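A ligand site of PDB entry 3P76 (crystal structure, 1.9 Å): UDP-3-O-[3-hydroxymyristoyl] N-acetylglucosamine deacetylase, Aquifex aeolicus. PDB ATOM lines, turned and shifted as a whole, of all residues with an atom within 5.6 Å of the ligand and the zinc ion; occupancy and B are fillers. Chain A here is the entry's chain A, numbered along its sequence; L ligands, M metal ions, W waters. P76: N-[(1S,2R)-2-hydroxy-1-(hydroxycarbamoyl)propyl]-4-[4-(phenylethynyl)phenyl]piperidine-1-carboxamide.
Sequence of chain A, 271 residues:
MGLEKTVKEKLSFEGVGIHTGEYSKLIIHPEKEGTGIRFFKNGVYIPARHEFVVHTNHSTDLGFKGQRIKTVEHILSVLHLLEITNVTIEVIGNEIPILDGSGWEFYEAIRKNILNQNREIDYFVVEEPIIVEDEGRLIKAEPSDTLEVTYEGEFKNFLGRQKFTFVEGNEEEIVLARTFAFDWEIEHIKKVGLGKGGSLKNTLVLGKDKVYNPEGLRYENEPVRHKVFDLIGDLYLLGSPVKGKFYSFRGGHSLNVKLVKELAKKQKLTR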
ATOM      1  N   ILE A  18      15.273  -3.443   8.999  1.00  0.00           N
ATOM      2  CA  ILE A  18      15.353  -3.840  10.414  1.00  0.00           C
ATOM      3  C   ILE A  18      14.532  -2.964  11.377  1.00  0.00           C
ATOM      4  O   ILE A  18      13.959  -3.473  12.344  1.00  0.00           O
ATOM      5  CB  ILE A  18      16.804  -4.036  10.905  1.00  0.00           C
ATOM      6  CG1 ILE A  18      16.862  -5.024  12.103  1.00  0.00           C
ATOM      7  CG2 ILE A  18      17.510  -2.701  11.204  1.00  0.00           C
ATOM      8  CD1 ILE A  18      18.170  -5.651  12.325  1.00  0.00           C
ATOM      9  N   HIS A  19      14.509  -1.643  11.129  1.00  0.00           N
ATOM     10  CA  HIS A  19      13.786  -0.742  12.036  1.00  0.00           C
ATOM     11  C   HIS A  19      12.327  -0.547  11.720  1.00  0.00           C
ATOM     12  O   HIS A  19      11.501  -0.625  12.625  1.00  0.00           O
ATOM     13  CB  HIS A  19      14.542   0.587  12.193  1.00  0.00           C
ATOM     14  CG  HIS A  19      15.811   0.455  12.962  1.00  0.00           C
ATOM     15  ND1 HIS A  19      15.831  -0.026  14.260  1.00  0.00           N
ATOM     16  CD2 HIS A  19      17.080   0.732  12.588  1.00  0.00           C
ATOM     17  CE1 HIS A  19      17.098  -0.046  14.628  1.00  0.00           C
ATOM     18  NE2 HIS A  19      17.892   0.390  13.654  1.00  0.00           N
ATOM     19  N   HIS A  58      20.649   3.955  17.114  1.00  0.00           N
ATOM     20  CA  HIS A  58      20.472   2.564  16.634  1.00  0.00           C
ATOM     21  C   HIS A  58      20.597   2.383  15.118  1.00  0.00           C
ATOM     22  O   HIS A  58      20.566   1.250  14.635  1.00  0.00           O
ATOM     23  CB  HIS A  58      19.214   1.877  17.229  1.00  0.00           C
ATOM     24  CG  HIS A  58      19.147   1.986  18.723  1.00  0.00           C
ATOM     25  ND1 HIS A  58      19.936   1.202  19.535  1.00  0.00           N
ATOM     26  CD2 HIS A  58      18.401   2.822  19.491  1.00  0.00           C
ATOM     27  CE1 HIS A  58      19.659   1.583  20.780  1.00  0.00           C
ATOM     28  NE2 HIS A  58      18.728   2.537  20.804  1.00  0.00           N
ATOM     29  N   SER A  59      20.792   3.489  14.390  1.00  0.00           N
ATOM     30  CA  SER A  59      21.005   3.519  12.930  1.00  0.00           C
ATOM     31  C   SER A  59      21.390   4.917  12.522  1.00  0.00           C
ATOM     32  O   SER A  59      21.099   5.874  13.225  1.00  0.00           O
ATOM     33  CB  SER A  59      19.753   3.081  12.173  1.00  0.00           C
ATOM     34  OG  SER A  59      18.704   4.029  12.247  1.00  0.00           O
ATOM     35  N   THR A  71      18.762   3.678   8.090  1.00  0.00           N
ATOM     36  CA  THR A  71      19.781   2.624   8.085  1.00  0.00           C
ATOM     37  C   THR A  71      20.655   2.595   6.825  1.00  0.00           C
ATOM     38  O   THR A  71      20.717   1.591   6.122  1.00  0.00           O
ATOM     39  CB  THR A  71      19.096   1.268   8.449  1.00  0.00           C
ATOM     40  OG1 THR A  71      18.050   1.535   9.399  1.00  0.00           O
ATOM     41  CG2 THR A  71      20.056   0.218   8.989  1.00  0.00           C
ATOM     42  N   GLU A  73      24.011   2.916   6.931  1.00  0.00           N
ATOM     43  CA  GLU A  73      25.368   2.475   7.314  1.00  0.00           C
ATOM     44  C   GLU A  73      25.988   1.254   6.623  1.00  0.00           C
ATOM     45  O   GLU A  73      27.163   1.293   6.286  1.00  0.00           O
ATOM     46  CB  GLU A  73      25.548   2.453   8.853  1.00  0.00           C
ATOM     47  CG  GLU A  73      24.635   1.465   9.549  1.00  0.00           C
ATOM     48  CD  GLU A  73      23.290   1.986  10.050  1.00  0.00           C
ATOM     49  OE1 GLU A  73      22.772   2.969   9.492  1.00  0.00           O
ATOM     50  OE2 GLU A  73      22.752   1.376  11.000  1.00  0.00           O
ATOM     51  N   HIS A  74      25.205   0.183   6.414  1.00  0.00           N
ATOM     52  CA  HIS A  74      25.715  -1.062   5.818  1.00  0.00           C
ATOM     53  C   HIS A  74      26.018  -0.923   4.336  1.00  0.00           C
ATOM     54  O   HIS A  74      27.096  -1.328   3.900  1.00  0.00           O
ATOM     55  CB  HIS A  74      24.777  -2.257   6.123  1.00  0.00           C
ATOM     56  CG  HIS A  74      24.501  -2.477   7.585  1.00  0.00           C
ATOM     57  ND1 HIS A  74      23.523  -3.356   7.998  1.00  0.00           N
ATOM     58  CD2 HIS A  74      25.109  -1.945   8.676  1.00  0.00           C
ATOM     59  CE1 HIS A  74      23.554  -3.336   9.326  1.00  0.00           C
ATOM     60  NE2 HIS A  74      24.478  -2.467   9.772  1.00  0.00           N
ATOM     61  N   GLY A 101      21.707  -9.156   7.835  1.00  0.00           N
ATOM     62  CA  GLY A 101      22.277  -8.354   8.913  1.00  0.00           C
ATOM     63  C   GLY A 101      23.702  -7.904   8.647  1.00  0.00           C
ATOM     64  O   GLY A 101      24.266  -7.126   9.412  1.00  0.00           O
ATOM     65  N   THR A 179      24.714  -7.441  12.288  1.00  0.00           N
ATOM     66  CA  THR A 179      24.194  -6.556  13.326  1.00  0.00           C
ATOM     67  C   THR A 179      23.794  -7.447  14.526  1.00  0.00           C
ATOM     68  O   THR A 179      23.499  -8.642  14.356  1.00  0.00           O
ATOM     69  CB  THR A 179      23.053  -5.664  12.805  1.00  0.00           C
ATOM     70  OG1 THR A 179      22.661  -4.789  13.868  1.00  0.00           O
ATOM     71  CG2 THR A 179      21.862  -6.441  12.311  1.00  0.00           C
ATOM     72  N   PHE A 180      23.875  -6.883  15.717  1.00  0.00           N
ATOM     73  CA  PHE A 180      23.607  -7.645  16.927  1.00  0.00           C
ATOM     74  C   PHE A 180      22.779  -6.858  17.914  1.00  0.00           C
ATOM     75  O   PHE A 180      22.666  -5.631  17.800  1.00  0.00           O
ATOM     76  CB  PHE A 180      24.924  -8.144  17.561  1.00  0.00           C
ATOM     77  CG  PHE A 180      25.841  -7.033  18.035  1.00  0.00           C
ATOM     78  CD1 PHE A 180      25.871  -6.663  19.366  1.00  0.00           C
ATOM     79  CD2 PHE A 180      26.704  -6.384  17.143  1.00  0.00           C
ATOM     80  CE1 PHE A 180      26.722  -5.642  19.815  1.00  0.00           C
ATOM     81  CE2 PHE A 180      27.517  -5.334  17.580  1.00  0.00           C
ATOM     82  CZ  PHE A 180      27.538  -4.983  18.910  1.00  0.00           C
ATOM     83  N   ALA A 181      22.194  -7.557  18.886  1.00  0.00           N
ATOM     84  CA  ALA A 181      21.379  -6.968  19.938  1.00  0.00           C
ATOM     85  C   ALA A 181      21.460  -7.802  21.198  1.00  0.00           C
ATOM     86  O   ALA A 181      21.693  -9.019  21.147  1.00  0.00           O
ATOM     87  CB  ALA A 181      19.925  -6.849  19.492  1.00  0.00           C
ATOM     88  N   ILE A 186      16.215  -5.084  23.967  1.00  0.00           N
ATOM     89  CA  ILE A 186      15.162  -5.177  22.948  1.00  0.00           C
ATOM     90  C   ILE A 186      13.857  -4.453  23.304  1.00  0.00           C
ATOM     91  O   ILE A 186      13.335  -3.733  22.466  1.00  0.00           O
ATOM     92  CB  ILE A 186      14.957  -6.640  22.421  1.00  0.00           C
ATOM     93  CG1 ILE A 186      16.249  -7.159  21.739  1.00  0.00           C
ATOM     94  CG2 ILE A 186      13.741  -6.728  21.460  1.00  0.00           C
ATOM     95  CD1 ILE A 186      16.298  -8.681  21.526  1.00  0.00           C
ATOM     96  N   ILE A 189      14.206  -0.763  22.658  1.00  0.00           N
ATOM     97  CA  ILE A 189      14.300  -0.510  21.216  1.00  0.00           C
ATOM     98  C   ILE A 189      12.894  -0.551  20.563  1.00  0.00           C
ATOM     99  O   ILE A 189      12.568   0.360  19.803  1.00  0.00           O
ATOM    100  CB  ILE A 189      15.352  -1.445  20.539  1.00  0.00           C
ATOM    101  CG1 ILE A 189      16.772  -1.109  21.068  1.00  0.00           C
ATOM    102  CG2 ILE A 189      15.297  -1.365  19.001  1.00  0.00           C
ATOM    103  CD1 ILE A 189      17.853  -2.202  20.916  1.00  0.00           C
ATOM    104  N   LYS A 190      12.064  -1.544  20.930  1.00  0.00           N
ATOM    105  CA  LYS A 190      10.698  -1.700  20.429  1.00  0.00           C
ATOM    106  C   LYS A 190       9.806  -0.553  20.943  1.00  0.00           C
ATOM    107  O   LYS A 190       8.990  -0.016  20.188  1.00  0.00           O
ATOM    108  CB  LYS A 190      10.086  -3.055  20.833  1.00  0.00           C
ATOM    109  CG  LYS A 190      10.838  -4.289  20.336  1.00  0.00           C
ATOM    110  CD  LYS A 190      10.570  -4.692  18.887  1.00  0.00           C
ATOM    111  CE  LYS A 190      10.928  -6.147  18.685  1.00  0.00           C
ATOM    112  NZ  LYS A 190      11.153  -6.495  17.257  1.00  0.00           N
ATOM    113  N   GLY A 195      13.476  -1.302  15.689  1.00  0.00           N
ATOM    114  CA  GLY A 195      13.705  -2.741  15.574  1.00  0.00           C
ATOM    115  C   GLY A 195      12.508  -3.595  15.176  1.00  0.00           C
ATOM    116  O   GLY A 195      12.471  -4.770  15.525  1.00  0.00           O
ATOM    117  N   GLY A 198      13.477  -6.724  13.128  1.00  0.00           N
ATOM    118  CA  GLY A 198      14.534  -7.500  13.765  1.00  0.00           C
ATOM    119  C   GLY A 198      14.080  -8.899  14.122  1.00  0.00           C
ATOM    120  O   GLY A 198      12.985  -9.071  14.655  1.00  0.00           O
ATOM    121  N   SER A 199      14.910  -9.897  13.791  1.00  0.00           N
ATOM    122  CA  SER A 199      14.611 -11.301  14.078  1.00  0.00           C
ATOM    123  C   SER A 199      15.911 -12.088  14.108  1.00  0.00           C
ATOM    124  O   SER A 199      16.963 -11.535  13.805  1.00  0.00           O
ATOM    125  CB  SER A 199      13.678 -11.869  13.001  1.00  0.00           C
ATOM    126  OG  SER A 199      14.360 -12.163  11.793  1.00  0.00           O
ATOM    127  N   LEU A 200      15.831 -13.393  14.431  1.00  0.00           N
ATOM    128  CA  LEU A 200      17.002 -14.269  14.439  1.00  0.00           C
ATOM    129  C   LEU A 200      17.533 -14.541  13.032  1.00  0.00           C
ATOM    130  O   LEU A 200      18.613 -15.092  12.884  1.00  0.00           O
ATOM    131  CB  LEU A 200      16.711 -15.572  15.212  1.00  0.00           C
ATOM    132  CG  LEU A 200      16.414 -15.429  16.713  1.00  0.00           C
ATOM    133  CD1 LEU A 200      16.129 -16.788  17.355  1.00  0.00           C
ATOM    134  CD2 LEU A 200      17.558 -14.730  17.447  1.00  0.00           C
ATOM    135  N   ASN A 202      18.078 -12.039  10.763  1.00  0.00           N
ATOM    136  CA  ASN A 202      18.897 -10.896  10.365  1.00  0.00           C
ATOM    137  C   ASN A 202      19.717 -10.284  11.512  1.00  0.00           C
ATOM    138  O   ASN A 202      20.434  -9.302  11.291  1.00  0.00           O
ATOM    139  CB  ASN A 202      18.014  -9.814   9.700  1.00  0.00           C
ATOM    140  CG  ASN A 202      16.835  -9.350  10.531  1.00  0.00           C
ATOM    141  OD1 ASN A 202      16.943  -9.106  11.735  1.00  0.00           O
ATOM    142  ND2 ASN A 202      15.694  -9.153   9.898  1.00  0.00           N
ATOM    143  N   THR A 203      19.602 -10.817  12.733  1.00  0.00           N
ATOM    144  CA  THR A 203      20.324 -10.283  13.898  1.00  0.00           C
ATOM    145  C   THR A 203      20.899 -11.372  14.769  1.00  0.00           C
ATOM    146  O   THR A 203      20.226 -12.371  15.055  1.00  0.00           O
ATOM    147  CB  THR A 203      19.392  -9.372  14.735  1.00  0.00           C
ATOM    148  OG1 THR A 203      18.805  -8.371  13.907  1.00  0.00           O
ATOM    149  CG2 THR A 203      20.108  -8.716  15.923  1.00  0.00           C
ATOM    150  N   VAL A 205      21.390 -12.332  18.230  1.00  0.00           N
ATOM    151  CA  VAL A 205      20.801 -11.965  19.512  1.00  0.00           C
ATOM    152  C   VAL A 205      21.476 -12.733  20.655  1.00  0.00           C
ATOM    153  O   VAL A 205      21.530 -13.965  20.648  1.00  0.00           O
ATOM    154  CB  VAL A 205      19.258 -12.064  19.531  1.00  0.00           C
ATOM    155  CG1 VAL A 205      18.709 -11.645  20.894  1.00  0.00           C
ATOM    156  CG2 VAL A 205      18.648 -11.216  18.413  1.00  0.00           C
ATOM    157  N   TYR A 212      21.010 -16.796  21.203  1.00  0.00           N
ATOM    158  CA  TYR A 212      19.671 -17.190  20.752  1.00  0.00           C
ATOM    159  C   TYR A 212      19.682 -17.883  19.386  1.00  0.00           C
ATOM    160  O   TYR A 212      18.920 -18.824  19.176  1.00  0.00           O
ATOM    161  CB  TYR A 212      18.741 -15.959  20.700  1.00  0.00           C
ATOM    162  CG  TYR A 212      18.236 -15.500  22.054  1.00  0.00           C
ATOM    163  CD1 TYR A 212      19.044 -14.771  22.911  1.00  0.00           C
ATOM    164  CD2 TYR A 212      16.911 -15.735  22.442  1.00  0.00           C
ATOM    165  CE1 TYR A 212      18.590 -14.347  24.156  1.00  0.00           C
ATOM    166  CE2 TYR A 212      16.438 -15.302  23.681  1.00  0.00           C
ATOM    167  CZ  TYR A 212      17.271 -14.603  24.526  1.00  0.00           C
ATOM    168  OH  TYR A 212      16.797 -14.142  25.732  1.00  0.00           O
ATOM    169  N   HIS A 226      31.400  -6.256  13.413  1.00  0.00           N
ATOM    170  CA  HIS A 226      30.249  -5.514  12.887  1.00  0.00           C
ATOM    171  C   HIS A 226      30.351  -4.038  13.228  1.00  0.00           C
ATOM    172  O   HIS A 226      30.002  -3.200  12.402  1.00  0.00           O
ATOM    173  CB  HIS A 226      28.899  -6.065  13.366  1.00  0.00           C
ATOM    174  CG  HIS A 226      27.760  -5.350  12.688  1.00  0.00           C
ATOM    175  ND1 HIS A 226      27.409  -5.645  11.387  1.00  0.00           N
ATOM    176  CD2 HIS A 226      27.040  -4.280  13.109  1.00  0.00           C
ATOM    177  CE1 HIS A 226      26.454  -4.787  11.056  1.00  0.00           C
ATOM    178  NE2 HIS A 226      26.191  -3.947  12.063  1.00  0.00           N
ATOM    179  N   LYS A 227      30.812  -3.719  14.433  1.00  0.00           N
ATOM    180  CA  LYS A 227      30.983  -2.330  14.860  1.00  0.00           C
ATOM    181  C   LYS A 227      32.053  -1.612  14.013  1.00  0.00           C
ATOM    182  O   LYS A 227      31.899  -0.422  13.713  1.00  0.00           O
ATOM    183  CB  LYS A 227      31.311  -2.286  16.354  1.00  0.00           C
ATOM    184  CG  LYS A 227      30.088  -2.509  17.269  1.00  0.00           C
ATOM    185  CD  LYS A 227      29.192  -1.262  17.351  1.00  0.00           C
ATOM    186  CE  LYS A 227      28.167  -1.338  18.449  1.00  0.00           C
ATOM    187  NZ  LYS A 227      27.333  -0.104  18.497  1.00  0.00           N
ATOM    188  N   PHE A 229      32.648  -2.418  10.788  1.00  0.00           N
ATOM    189  CA  PHE A 229      31.873  -2.294   9.555  1.00  0.00           C
ATOM    190  C   PHE A 229      30.910  -1.067   9.619  1.00  0.00           C
ATOM    191  O   PHE A 229      30.855  -0.278   8.670  1.00  0.00           O
ATOM    192  CB  PHE A 229      31.147  -3.618   9.292  1.00  0.00           C
ATOM    193  CG  PHE A 229      30.238  -3.650   8.091  1.00  0.00           C
ATOM    194  CD1 PHE A 229      30.745  -3.796   6.806  1.00  0.00           C
ATOM    195  CD2 PHE A 229      28.856  -3.565   8.239  1.00  0.00           C
ATOM    196  CE1 PHE A 229      29.904  -3.805   5.696  1.00  0.00           C
ATOM    197  CE2 PHE A 229      28.012  -3.594   7.140  1.00  0.00           C
ATOM    198  CZ  PHE A 229      28.536  -3.709   5.868  1.00  0.00           C
ATOM    199  N   ASP A 230      30.245  -0.875  10.764  1.00  0.00           N
ATOM    200  CA  ASP A 230      29.349   0.278  10.996  1.00  0.00           C
ATOM    201  C   ASP A 230      30.103   1.606  10.903  1.00  0.00           C
ATOM    202  O   ASP A 230      29.636   2.532  10.238  1.00  0.00           O
ATOM    203  CB  ASP A 230      28.679   0.180  12.383  1.00  0.00           C
ATOM    204  CG  ASP A 230      27.475  -0.732  12.453  1.00  0.00           C
ATOM    205  OD1 ASP A 230      26.937  -1.095  11.373  1.00  0.00           O
ATOM    206  OD2 ASP A 230      27.011  -1.015  13.585  1.00  0.00           O
ATOM    207  N   HIS A 253      26.850   5.154  16.417  1.00  0.00           N
ATOM    208  CA  HIS A 253      26.578   6.098  15.317  1.00  0.00           C
ATOM    209  C   HIS A 253      26.651   7.567  15.722  1.00  0.00           C
ATOM    210  O   HIS A 253      27.188   8.366  14.960  1.00  0.00           O
ATOM    211  CB  HIS A 253      25.248   5.803  14.614  1.00  0.00           C
ATOM    212  CG  HIS A 253      25.155   4.399  14.095  1.00  0.00           C
ATOM    213  ND1 HIS A 253      25.983   3.951  13.071  1.00  0.00           N
ATOM    214  CD2 HIS A 253      24.340   3.386  14.478  1.00  0.00           C
ATOM    215  CE1 HIS A 253      25.634   2.685  12.869  1.00  0.00           C
ATOM    216  NE2 HIS A 253      24.673   2.305  13.699  1.00  0.00           N
HETATM  217  N1  P76 L   1      21.995  -2.176  15.424  1.00  0.00           N
HETATM  218  C2  P76 L   1      23.300  -1.552  15.438  1.00  0.00           C
HETATM  219  C3  P76 L   1      23.710  -1.494  13.980  1.00  0.00           C
HETATM  220  O4  P76 L   1      23.999  -2.499  13.320  1.00  0.00           O
HETATM  221  N5  P76 L   1      23.731  -0.203  13.537  1.00  0.00           N
HETATM  222  O6  P76 L   1      24.135  -0.168  12.214  1.00  0.00           O
HETATM  223  C7  P76 L   1      21.106  -1.995  16.517  1.00  0.00           C
HETATM  224  O8  P76 L   1      21.395  -1.302  17.521  1.00  0.00           O
HETATM  225  N9  P76 L   1      19.887  -2.646  16.383  1.00  0.00           N
HETATM  226  C10 P76 L   1      19.468  -3.434  15.212  1.00  0.00           C
HETATM  227  C11 P76 L   1      18.829  -4.728  15.637  1.00  0.00           C
HETATM  228  C12 P76 L   1      17.561  -4.444  16.452  1.00  0.00           C
HETATM  229  C13 P76 L   1      18.043  -3.741  17.728  1.00  0.00           C
HETATM  230  C14 P76 L   1      18.886  -2.493  17.467  1.00  0.00           C
HETATM  231  C15 P76 L   1      16.813  -5.707  16.855  1.00  0.00           C
HETATM  232  C16 P76 L   1      15.670  -5.673  17.707  1.00  0.00           C
HETATM  233  C17 P76 L   1      15.007  -6.869  18.068  1.00  0.00           C
HETATM  234  C18 P76 L   1      15.490  -8.100  17.568  1.00  0.00           C
HETATM  235  C19 P76 L   1      16.596  -8.162  16.738  1.00  0.00           C
HETATM  236  C20 P76 L   1      17.224  -6.985  16.389  1.00  0.00           C
HETATM  237  C21 P76 L   1      14.944  -9.350  17.882  1.00  0.00           C
HETATM  238  C22 P76 L   1      14.670 -10.440  18.264  1.00  0.00           C
HETATM  239  C23 P76 L   1      14.353 -11.736  18.728  1.00  0.00           C
HETATM  240  C24 P76 L   1      14.783 -12.072  20.040  1.00  0.00           C
HETATM  241  C25 P76 L   1      14.488 -13.346  20.571  1.00  0.00           C
HETATM  242  C26 P76 L   1      13.775 -14.273  19.782  1.00  0.00           C
HETATM  243  C27 P76 L   1      13.354 -13.927  18.472  1.00  0.00           C
HETATM  244  C28 P76 L   1      13.640 -12.644  17.937  1.00  0.00           C
HETATM  245  C29 P76 L   1      24.358  -2.174  16.369  1.00  0.00           C
HETATM  246  C30 P76 L   1      24.606  -3.659  16.148  1.00  0.00           C
HETATM  247  O31 P76 L   1      25.586  -1.460  16.138  1.00  0.00           O
HETATM  248 ZN    ZN M   1      25.276  -2.157  11.738  1.00  0.00          ZN
HETATM  249  O   HOH W   1      21.187  -2.820  12.056  1.00  0.00           O
HETATM  250  O   HOH W   2      20.718  -0.207  12.357  1.00  0.00           O
HETATM  251  O   HOH W   3      22.847  -3.465  19.669  1.00  0.00           O
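N5 of the ligand sits at hydrogen-bond distance from OE2 of Glu 73 (3.1 Å).
A ring nitrogen (NE2) of His 253 sits at hydrogen-bond distance from a nitrogen (N5) of the ligand.
OG1 of Thr 179 is in hydrogen-bond range of N1 of the ligand (3.1 Å).
NZ of Lys 227 is in hydrogen-bond range of O31 of the ligand, 3.2 Å away.
Within 4 Å of the zinc ion: His 74, His 226 and Asp 230.
The nearest printed residue that does not touch the zinc ion is Thr 179 (4.3 Å).
The zinc ion is bound by the side-chain carboxylate of Asp 230 (2.0 Å), a ring nitrogen (NE2) of His 226 (2.0 Å), an oxygen (O4) of the ligand (2.1 Å), a ring nitrogen (NE2) of His 74 (2.1 Å) and an oxygen (O6) of the ligand (2.3 Å).
The zinc ion has five donor atoms within binding distance.
Slightly farther from the zinc ion lies the side-chain carboxylate (OD2) of Asp 230 (2.8 Å).
Water W2 lies within hydrogen-bond range of O of His 58 (2.7 Å), OE2 of Glu 73 (2.9 Å), NE2 of His 19 (3.2 Å) and N5 of the ligand (3.2 Å).
Water W3 lies within hydrogen-bond range of the backbone carbonyl oxygen of Phe 180 and an oxygen (O8) of the ligand.
Merely in contact with the ligand: Ile 18, His 58, Phe 180, Ile 186, Ile 189, Lys 190, Gly 195, Gly 198, Ser 199, Leu 200, Thr 203 and Tyr 212.
Within 4 Å of the ligand: Ile 18, His 58, Glu 73, His 74, Thr 179, Phe 180, Ile 186, Ile 189, Lys 190, Gly 195, Gly 198, Ser 199, Leu 200, Thr 203, Tyr 212, His 226, Lys 227, Asp 230 and His 253.
The nearest printed residue that does not touch the ligand is Ala 181 (4.04 Å).
A ring nitrogen (ND1) of His 226 sits at hydrogen-bond distance from the backbone NH of Thr 179.
The side-chain carboxylate (OE2) of Glu 73 lies within hydrogen-bond range of a ring nitrogen (NE2) of His 253 (3.4 Å).
The backbone NH of Gly 195 is in hydrogen-bond range of a ring nitrogen (ND1) of His 19 (3.0 Å).
O of His 58 is in hydrogen-bond range of NE2 of His 19 (3.0 Å).
The side-chain amide oxygen of Asn 202 lies within hydrogen-bond range of the side-chain hydroxyl of Thr 203, 3.0 Å away.
The backbone NH (N) of Thr 179 sits at hydrogen-bond distance from the backbone carbonyl oxygen (O) of Gly 101 (2.9 Å).
The backbone NH (N) of Gly 198 lies within hydrogen-bond range of the backbone carbonyl oxygen (O) of Ile 18 (3.4 Å).
The backbone NH (N) of Ser 199 lies within hydrogen-bond range of the side-chain amide oxygen (OD1) of Asn 202 (3.0 Å).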
